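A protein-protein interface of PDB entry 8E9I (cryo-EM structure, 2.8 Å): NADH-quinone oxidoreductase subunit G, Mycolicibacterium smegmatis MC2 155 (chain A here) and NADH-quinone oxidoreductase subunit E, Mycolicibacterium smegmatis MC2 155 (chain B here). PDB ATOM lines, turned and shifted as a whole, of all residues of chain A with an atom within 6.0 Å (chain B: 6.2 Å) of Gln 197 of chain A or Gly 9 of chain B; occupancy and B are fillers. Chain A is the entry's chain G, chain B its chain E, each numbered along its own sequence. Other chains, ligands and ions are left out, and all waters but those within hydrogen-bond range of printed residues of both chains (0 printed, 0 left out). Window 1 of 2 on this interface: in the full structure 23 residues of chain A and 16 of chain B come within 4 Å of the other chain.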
ATOM      1  N   ILE A 150       7.887  18.268  10.995  1.00  0.00           N
ATOM      2  CA  ILE A 150       8.959  19.001  11.650  1.00  0.00           C
ATOM      3  C   ILE A 150       9.890  19.541  10.578  1.00  0.00           C
ATOM      4  O   ILE A 150      10.293  18.810   9.668  1.00  0.00           O
ATOM      5  CB  ILE A 150       9.730  18.129  12.659  1.00  0.00           C
ATOM      6  CG1 ILE A 150      10.475  17.000  11.951  1.00  0.00           C
ATOM      7  CG2 ILE A 150       8.784  17.565  13.692  1.00  0.00           C
ATOM      8  CD1 ILE A 150      11.354  16.205  12.870  1.00  0.00           C
ATOM      9  N   SER A 151      10.217  20.821  10.678  1.00  0.00           N
ATOM     10  CA  SER A 151      11.123  21.423   9.716  1.00  0.00           C
ATOM     11  C   SER A 151      12.544  20.963   9.992  1.00  0.00           C
ATOM     12  O   SER A 151      13.008  20.999  11.133  1.00  0.00           O
ATOM     13  CB  SER A 151      11.040  22.943   9.788  1.00  0.00           C
ATOM     14  OG  SER A 151       9.696  23.375   9.747  1.00  0.00           O
ATOM     15  N   ILE A 152      13.227  20.504   8.946  1.00  0.00           N
ATOM     16  CA  ILE A 152      14.666  20.297   9.012  1.00  0.00           C
ATOM     17  C   ILE A 152      15.420  21.438   8.355  1.00  0.00           C
ATOM     18  O   ILE A 152      16.658  21.395   8.287  1.00  0.00           O
ATOM     19  CB  ILE A 152      15.067  18.949   8.381  1.00  0.00           C
ATOM     20  CG1 ILE A 152      14.448  18.797   6.999  1.00  0.00           C
ATOM     21  CG2 ILE A 152      14.621  17.813   9.265  1.00  0.00           C
ATOM     22  CD1 ILE A 152      15.092  17.725   6.173  1.00  0.00           C
ATOM     23  N   ILE A 195      17.887  15.889  11.414  1.00  0.00           N
ATOM     24  CA  ILE A 195      19.018  16.802  11.508  1.00  0.00           C
ATOM     25  C   ILE A 195      19.607  16.658  12.900  1.00  0.00           C
ATOM     26  O   ILE A 195      19.023  15.988  13.757  1.00  0.00           O
ATOM     27  CB  ILE A 195      18.605  18.253  11.219  1.00  0.00           C
ATOM     28  CG1 ILE A 195      17.412  18.652  12.080  1.00  0.00           C
ATOM     29  CG2 ILE A 195      18.296  18.422   9.745  1.00  0.00           C
ATOM     30  CD1 ILE A 195      17.199  20.130  12.146  1.00  0.00           C
ATOM     31  N   GLY A 196      20.767  17.260  13.141  1.00  0.00           N
ATOM     32  CA  GLY A 196      21.457  16.951  14.373  1.00  0.00           C
ATOM     33  C   GLY A 196      20.645  17.283  15.606  1.00  0.00           C
ATOM     34  O   GLY A 196      20.065  16.383  16.218  1.00  0.00           O
ATOM     35  N   GLN A 197      20.571  18.557  15.980  1.00  0.00           N
ATOM     36  CA  GLN A 197      19.666  18.964  17.045  1.00  0.00           C
ATOM     37  C   GLN A 197      18.756  20.082  16.572  1.00  0.00           C
ATOM     38  O   GLN A 197      17.527  19.960  16.585  1.00  0.00           O
ATOM     39  CB  GLN A 197      20.466  19.399  18.271  1.00  0.00           C
ATOM     40  CG  GLN A 197      20.981  18.229  19.073  1.00  0.00           C
ATOM     41  CD  GLN A 197      22.049  17.450  18.340  1.00  0.00           C
ATOM     42  OE1 GLN A 197      22.979  18.025  17.777  1.00  0.00           O
ATOM     43  NE2 GLN A 197      21.898  16.133  18.308  1.00  0.00           N
ATOM     44  N   ASP A 198      19.379  21.173  16.140  1.00  0.00           N
ATOM     45  CA  ASP A 198      18.712  22.309  15.527  1.00  0.00           C
ATOM     46  C   ASP A 198      19.460  22.832  14.316  1.00  0.00           C
ATOM     47  O   ASP A 198      18.908  23.634  13.563  1.00  0.00           O
ATOM     48  CB  ASP A 198      18.549  23.443  16.544  1.00  0.00           C
ATOM     49  N   LYS A 199      20.702  22.406  14.127  1.00  0.00           N
ATOM     50  CA  LYS A 199      21.447  22.740  12.928  1.00  0.00           C
ATOM     51  C   LYS A 199      20.604  22.389  11.709  1.00  0.00           C
ATOM     52  O   LYS A 199      20.337  21.201  11.474  1.00  0.00           O
ATOM     53  CB  LYS A 199      22.769  21.978  12.901  1.00  0.00           C
ATOM     54  N   GLU B   7      11.452  26.093  14.760  1.00  0.00           N
ATOM     55  CA  GLU B   7      11.273  24.799  15.412  1.00  0.00           C
ATOM     56  C   GLU B   7      11.923  23.686  14.585  1.00  0.00           C
ATOM     57  O   GLU B   7      11.298  22.695  14.205  1.00  0.00           O
ATOM     58  CB  GLU B   7       9.786  24.511  15.648  1.00  0.00           C
ATOM     59  N   LEU B   8      13.209  23.887  14.315  1.00  0.00           N
ATOM     60  CA  LEU B   8      13.988  22.879  13.614  1.00  0.00           C
ATOM     61  C   LEU B   8      14.339  21.730  14.552  1.00  0.00           C
ATOM     62  O   LEU B   8      14.662  21.941  15.723  1.00  0.00           O
ATOM     63  CB  LEU B   8      15.263  23.495  13.045  1.00  0.00           C
ATOM     64  CG  LEU B   8      15.054  24.530  11.942  1.00  0.00           C
ATOM     65  CD1 LEU B   8      16.261  25.435  11.838  1.00  0.00           C
ATOM     66  CD2 LEU B   8      14.785  23.857  10.621  1.00  0.00           C
ATOM     67  N   GLY B   9      14.275  20.508  14.028  1.00  0.00           N
ATOM     68  CA  GLY B   9      14.604  19.331  14.803  1.00  0.00           C
ATOM     69  C   GLY B   9      13.408  18.772  15.548  1.00  0.00           C
ATOM     70  O   GLY B   9      12.322  19.351  15.586  1.00  0.00           O
ATOM     71  N   GLN B  10      13.627  17.612  16.163  1.00  0.00           N
ATOM     72  CA  GLN B  10      12.552  16.925  16.864  1.00  0.00           C
ATOM     73  C   GLN B  10      11.965  17.810  17.954  1.00  0.00           C
ATOM     74  O   GLN B  10      12.631  18.699  18.492  1.00  0.00           O
ATOM     75  CB  GLN B  10      13.055  15.627  17.495  1.00  0.00           C
ATOM     76  CG  GLN B  10      13.745  14.666  16.552  1.00  0.00           C
ATOM     77  CD  GLN B  10      14.091  13.357  17.232  1.00  0.00           C
ATOM     78  OE1 GLN B  10      13.285  12.801  17.975  1.00  0.00           O
ATOM     79  NE2 GLN B  10      15.298  12.868  16.994  1.00  0.00           N
ATOM     80  N   ARG B  11      10.702  17.561  18.276  1.00  0.00           N
ATOM     81  CA  ARG B  11      10.089  18.226  19.410  1.00  0.00           C
ATOM     82  C   ARG B  11      10.753  17.746  20.700  1.00  0.00           C
ATOM     83  O   ARG B  11      11.087  16.564  20.822  1.00  0.00           O
ATOM     84  CB  ARG B  11       8.590  17.941  19.453  1.00  0.00           C
ATOM     85  CG  ARG B  11       7.860  18.214  18.145  1.00  0.00           C
ATOM     86  CD  ARG B  11       7.948  19.677  17.745  1.00  0.00           C
ATOM     87  NE  ARG B  11       7.323  19.930  16.453  1.00  0.00           N
ATOM     88  CZ  ARG B  11       6.015  19.931  16.235  1.00  0.00           C
ATOM     89  NH1 ARG B  11       5.151  19.683  17.206  1.00  0.00           N
ATOM     90  NH2 ARG B  11       5.563  20.179  15.009  1.00  0.00           N
ATOM     91  N   ILE B  19      18.685  14.287  22.001  1.00  0.00           N
ATOM     92  CA  ILE B  19      19.873  14.892  22.584  1.00  0.00           C
ATOM     93  C   ILE B  19      19.577  16.355  22.867  1.00  0.00           C
ATOM     94  O   ILE B  19      19.315  17.139  21.947  1.00  0.00           O
ATOM     95  CB  ILE B  19      21.074  14.733  21.649  1.00  0.00           C
ATOM     96  CG1 ILE B  19      21.393  13.254  21.425  1.00  0.00           C
ATOM     97  CG2 ILE B  19      22.273  15.458  22.211  1.00  0.00           C
ATOM     98  CD1 ILE B  19      22.011  12.570  22.616  1.00  0.00           C
ATOM     99  N   SER B  20      19.616  16.731  24.141  1.00  0.00           N
ATOM    100  CA  SER B  20      19.309  18.093  24.554  1.00  0.00           C
ATOM    101  C   SER B  20      20.096  18.396  25.819  1.00  0.00           C
ATOM    102  O   SER B  20      20.505  17.493  26.551  1.00  0.00           O
ATOM    103  CB  SER B  20      17.808  18.280  24.784  1.00  0.00           C
ATOM    104  OG  SER B  20      17.308  17.301  25.674  1.00  0.00           O
ATOM    105  N   PRO B  67      24.013  18.161  23.447  1.00  0.00           N
ATOM    106  CA  PRO B  67      24.484  18.807  22.218  1.00  0.00           C
ATOM    107  C   PRO B  67      25.921  19.270  22.304  1.00  0.00           C
ATOM    108  O   PRO B  67      26.621  19.261  21.287  1.00  0.00           O
ATOM    109  CB  PRO B  67      23.519  19.986  22.054  1.00  0.00           C
ATOM    110  CG  PRO B  67      22.296  19.567  22.763  1.00  0.00           C
ATOM    111  CD  PRO B  67      22.735  18.722  23.909  1.00  0.00           C
ATOM    112  N   ILE B  70      28.027  16.317  21.407  1.00  0.00           N
ATOM    113  CA  ILE B  70      27.912  16.060  19.975  1.00  0.00           C
ATOM    114  C   ILE B  70      28.784  17.033  19.196  1.00  0.00           C
ATOM    115  O   ILE B  70      29.507  16.648  18.270  1.00  0.00           O
ATOM    116  CB  ILE B  70      26.440  16.156  19.537  1.00  0.00           C
ATOM    117  CG1 ILE B  70      25.593  15.111  20.267  1.00  0.00           C
ATOM    118  CG2 ILE B  70      26.323  15.989  18.036  1.00  0.00           C
ATOM    119  CD1 ILE B  70      25.973  13.683  19.970  1.00  0.00           C
ATOM    120  N   GLY B  71      28.724  18.313  19.560  1.00  0.00           N
ATOM    121  CA  GLY B  71      29.538  19.301  18.882  1.00  0.00           C
ATOM    122  C   GLY B  71      31.020  19.049  19.045  1.00  0.00           C
ATOM    123  O   GLY B  71      31.783  19.179  18.087  1.00  0.00           O
ATOM    124  N   GLU B  81      27.375  17.480  12.929  1.00  0.00           N
ATOM    125  CA  GLU B  81      26.582  17.151  14.106  1.00  0.00           C
ATOM    126  C   GLU B  81      25.521  16.112  13.782  1.00  0.00           C
ATOM    127  O   GLU B  81      25.172  15.294  14.638  1.00  0.00           O
ATOM    128  CB  GLU B  81      25.936  18.414  14.673  1.00  0.00           C
ATOM    129  N   ALA B  82      24.999  16.118  12.557  1.00  0.00           N
ATOM    130  CA  ALA B  82      23.988  15.134  12.190  1.00  0.00           C
ATOM    131  C   ALA B  82      24.557  13.722  12.202  1.00  0.00           C
ATOM    132  O   ALA B  82      23.925  12.803  12.727  1.00  0.00           O
ATOM    133  CB  ALA B  82      23.409  15.462  10.818  1.00  0.00           C
ATOM    134  N   THR B  85      25.205  12.643  15.771  1.00  0.00           N
ATOM    135  CA  THR B  85      23.942  12.319  16.420  1.00  0.00           C
ATOM    136  C   THR B  85      23.420  10.971  15.952  1.00  0.00           C
ATOM    137  O   THR B  85      22.941  10.166  16.757  1.00  0.00           O
ATOM    138  CB  THR B  85      22.912  13.405  16.133  1.00  0.00           C
ATOM    139  OG1 THR B  85      23.423  14.673  16.557  1.00  0.00           O
ATOM    140  CG2 THR B  85      21.614  13.114  16.856  1.00  0.00           C
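Ile 150 of chain A touches Arg 11 of chain B (CG2 to NE, 3.9 Å).
Glu 7 of chain B touches Ser 151 of chain A (O to O, 3.9 Å).
Ser 151 of chain A touches Leu 8 of chain B (O to CA, 3.3 Å).
Ile 152 of chain A touches Leu 8 of chain B.
Leu 8 of chain B touches Ile 195 of chain A (CB to CD1, 3.98 Å).
Gly 196 of chain A touches Ala 82 of chain B.
O of Gly 196 of chain A touches CG2 of Thr 85 of chain B, 3.7 Å away.
Gly 9 of chain B touches Gln 197 of chain A.
CG of Gln 197 of chain A touches O of Ile 19 of chain B (3.5 Å).
Gln 197 of chain A touches Ile 70 of chain B (OE1 to CG2, 3.9 Å).
O of Glu 81 of chain B lies within hydrogen-bond range of OG1 of Thr 85 of chain B (2.7 Å).
Gln 197 of chain A touches five residues of chain B.
Gly 9 of chain B touches just these residues of chain A: Ser 151, Ile 195 and Gln 197.
Of the printed residues of chain A, Ile 70 of chain B touches Gln 197.
Of the printed residues of chain A, Thr 85 of chain B touches Gly 196 (3.7 Å) and Gln 197 (2.7 Å).
Of the printed residues of chain A, Ala 82 of chain B touches Gly 196 (3.8 Å).
Of the printed residues of chain A, Leu 8 of chain B touches Ser 151, Ile 152, Ile 195, Gln 197 and Asp 198.
Of the printed residues of chain A, Arg 11 of chain B touches Ile 150.
Ser 20 of chain B touches none of the printed residues of chain A.
Gln 10 of chain B touches none of the printed residues of chain A.
The nearest residue of chain B that does not touch Gln 197 of chain A is Pro 67 of chain B (4.1 Å).
The nearest residue of chain A that does not touch Gly 9 of chain B is Ile 150 of chain A (4.1 Å).
The nearest printed residue of chain A that does not touch Ile 19 of chain B is Gly 196 of chain A (5.8 Å).
Hydrophobic or aromatic side chains of chain B within 4 Å of the printed part of chain A: Leu 8, Ile 19, Ile 70 and Ala 82.
Of the 8 printed residues of chain A, 7 touch a printed residue of chain B.
Hydrophobic or aromatic side chains of chain A that line the printed part of chain B: Ile 150 and Ile 195.
Among the printed residues, no Asp or Glu carboxylate lies within 4 Å of a Lys or Arg side-chain nitrogen of the other chain.
N of Gly 9 of chain B is in hydrogen-bond range of O of Ser 151 of chain A (3.2 Å).
The side-chain amide nitrogen (NE2) of Gln 197 of chain A is in hydrogen-bond range of the side-chain hydroxyl (OG1) of Thr 85 of chain B.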
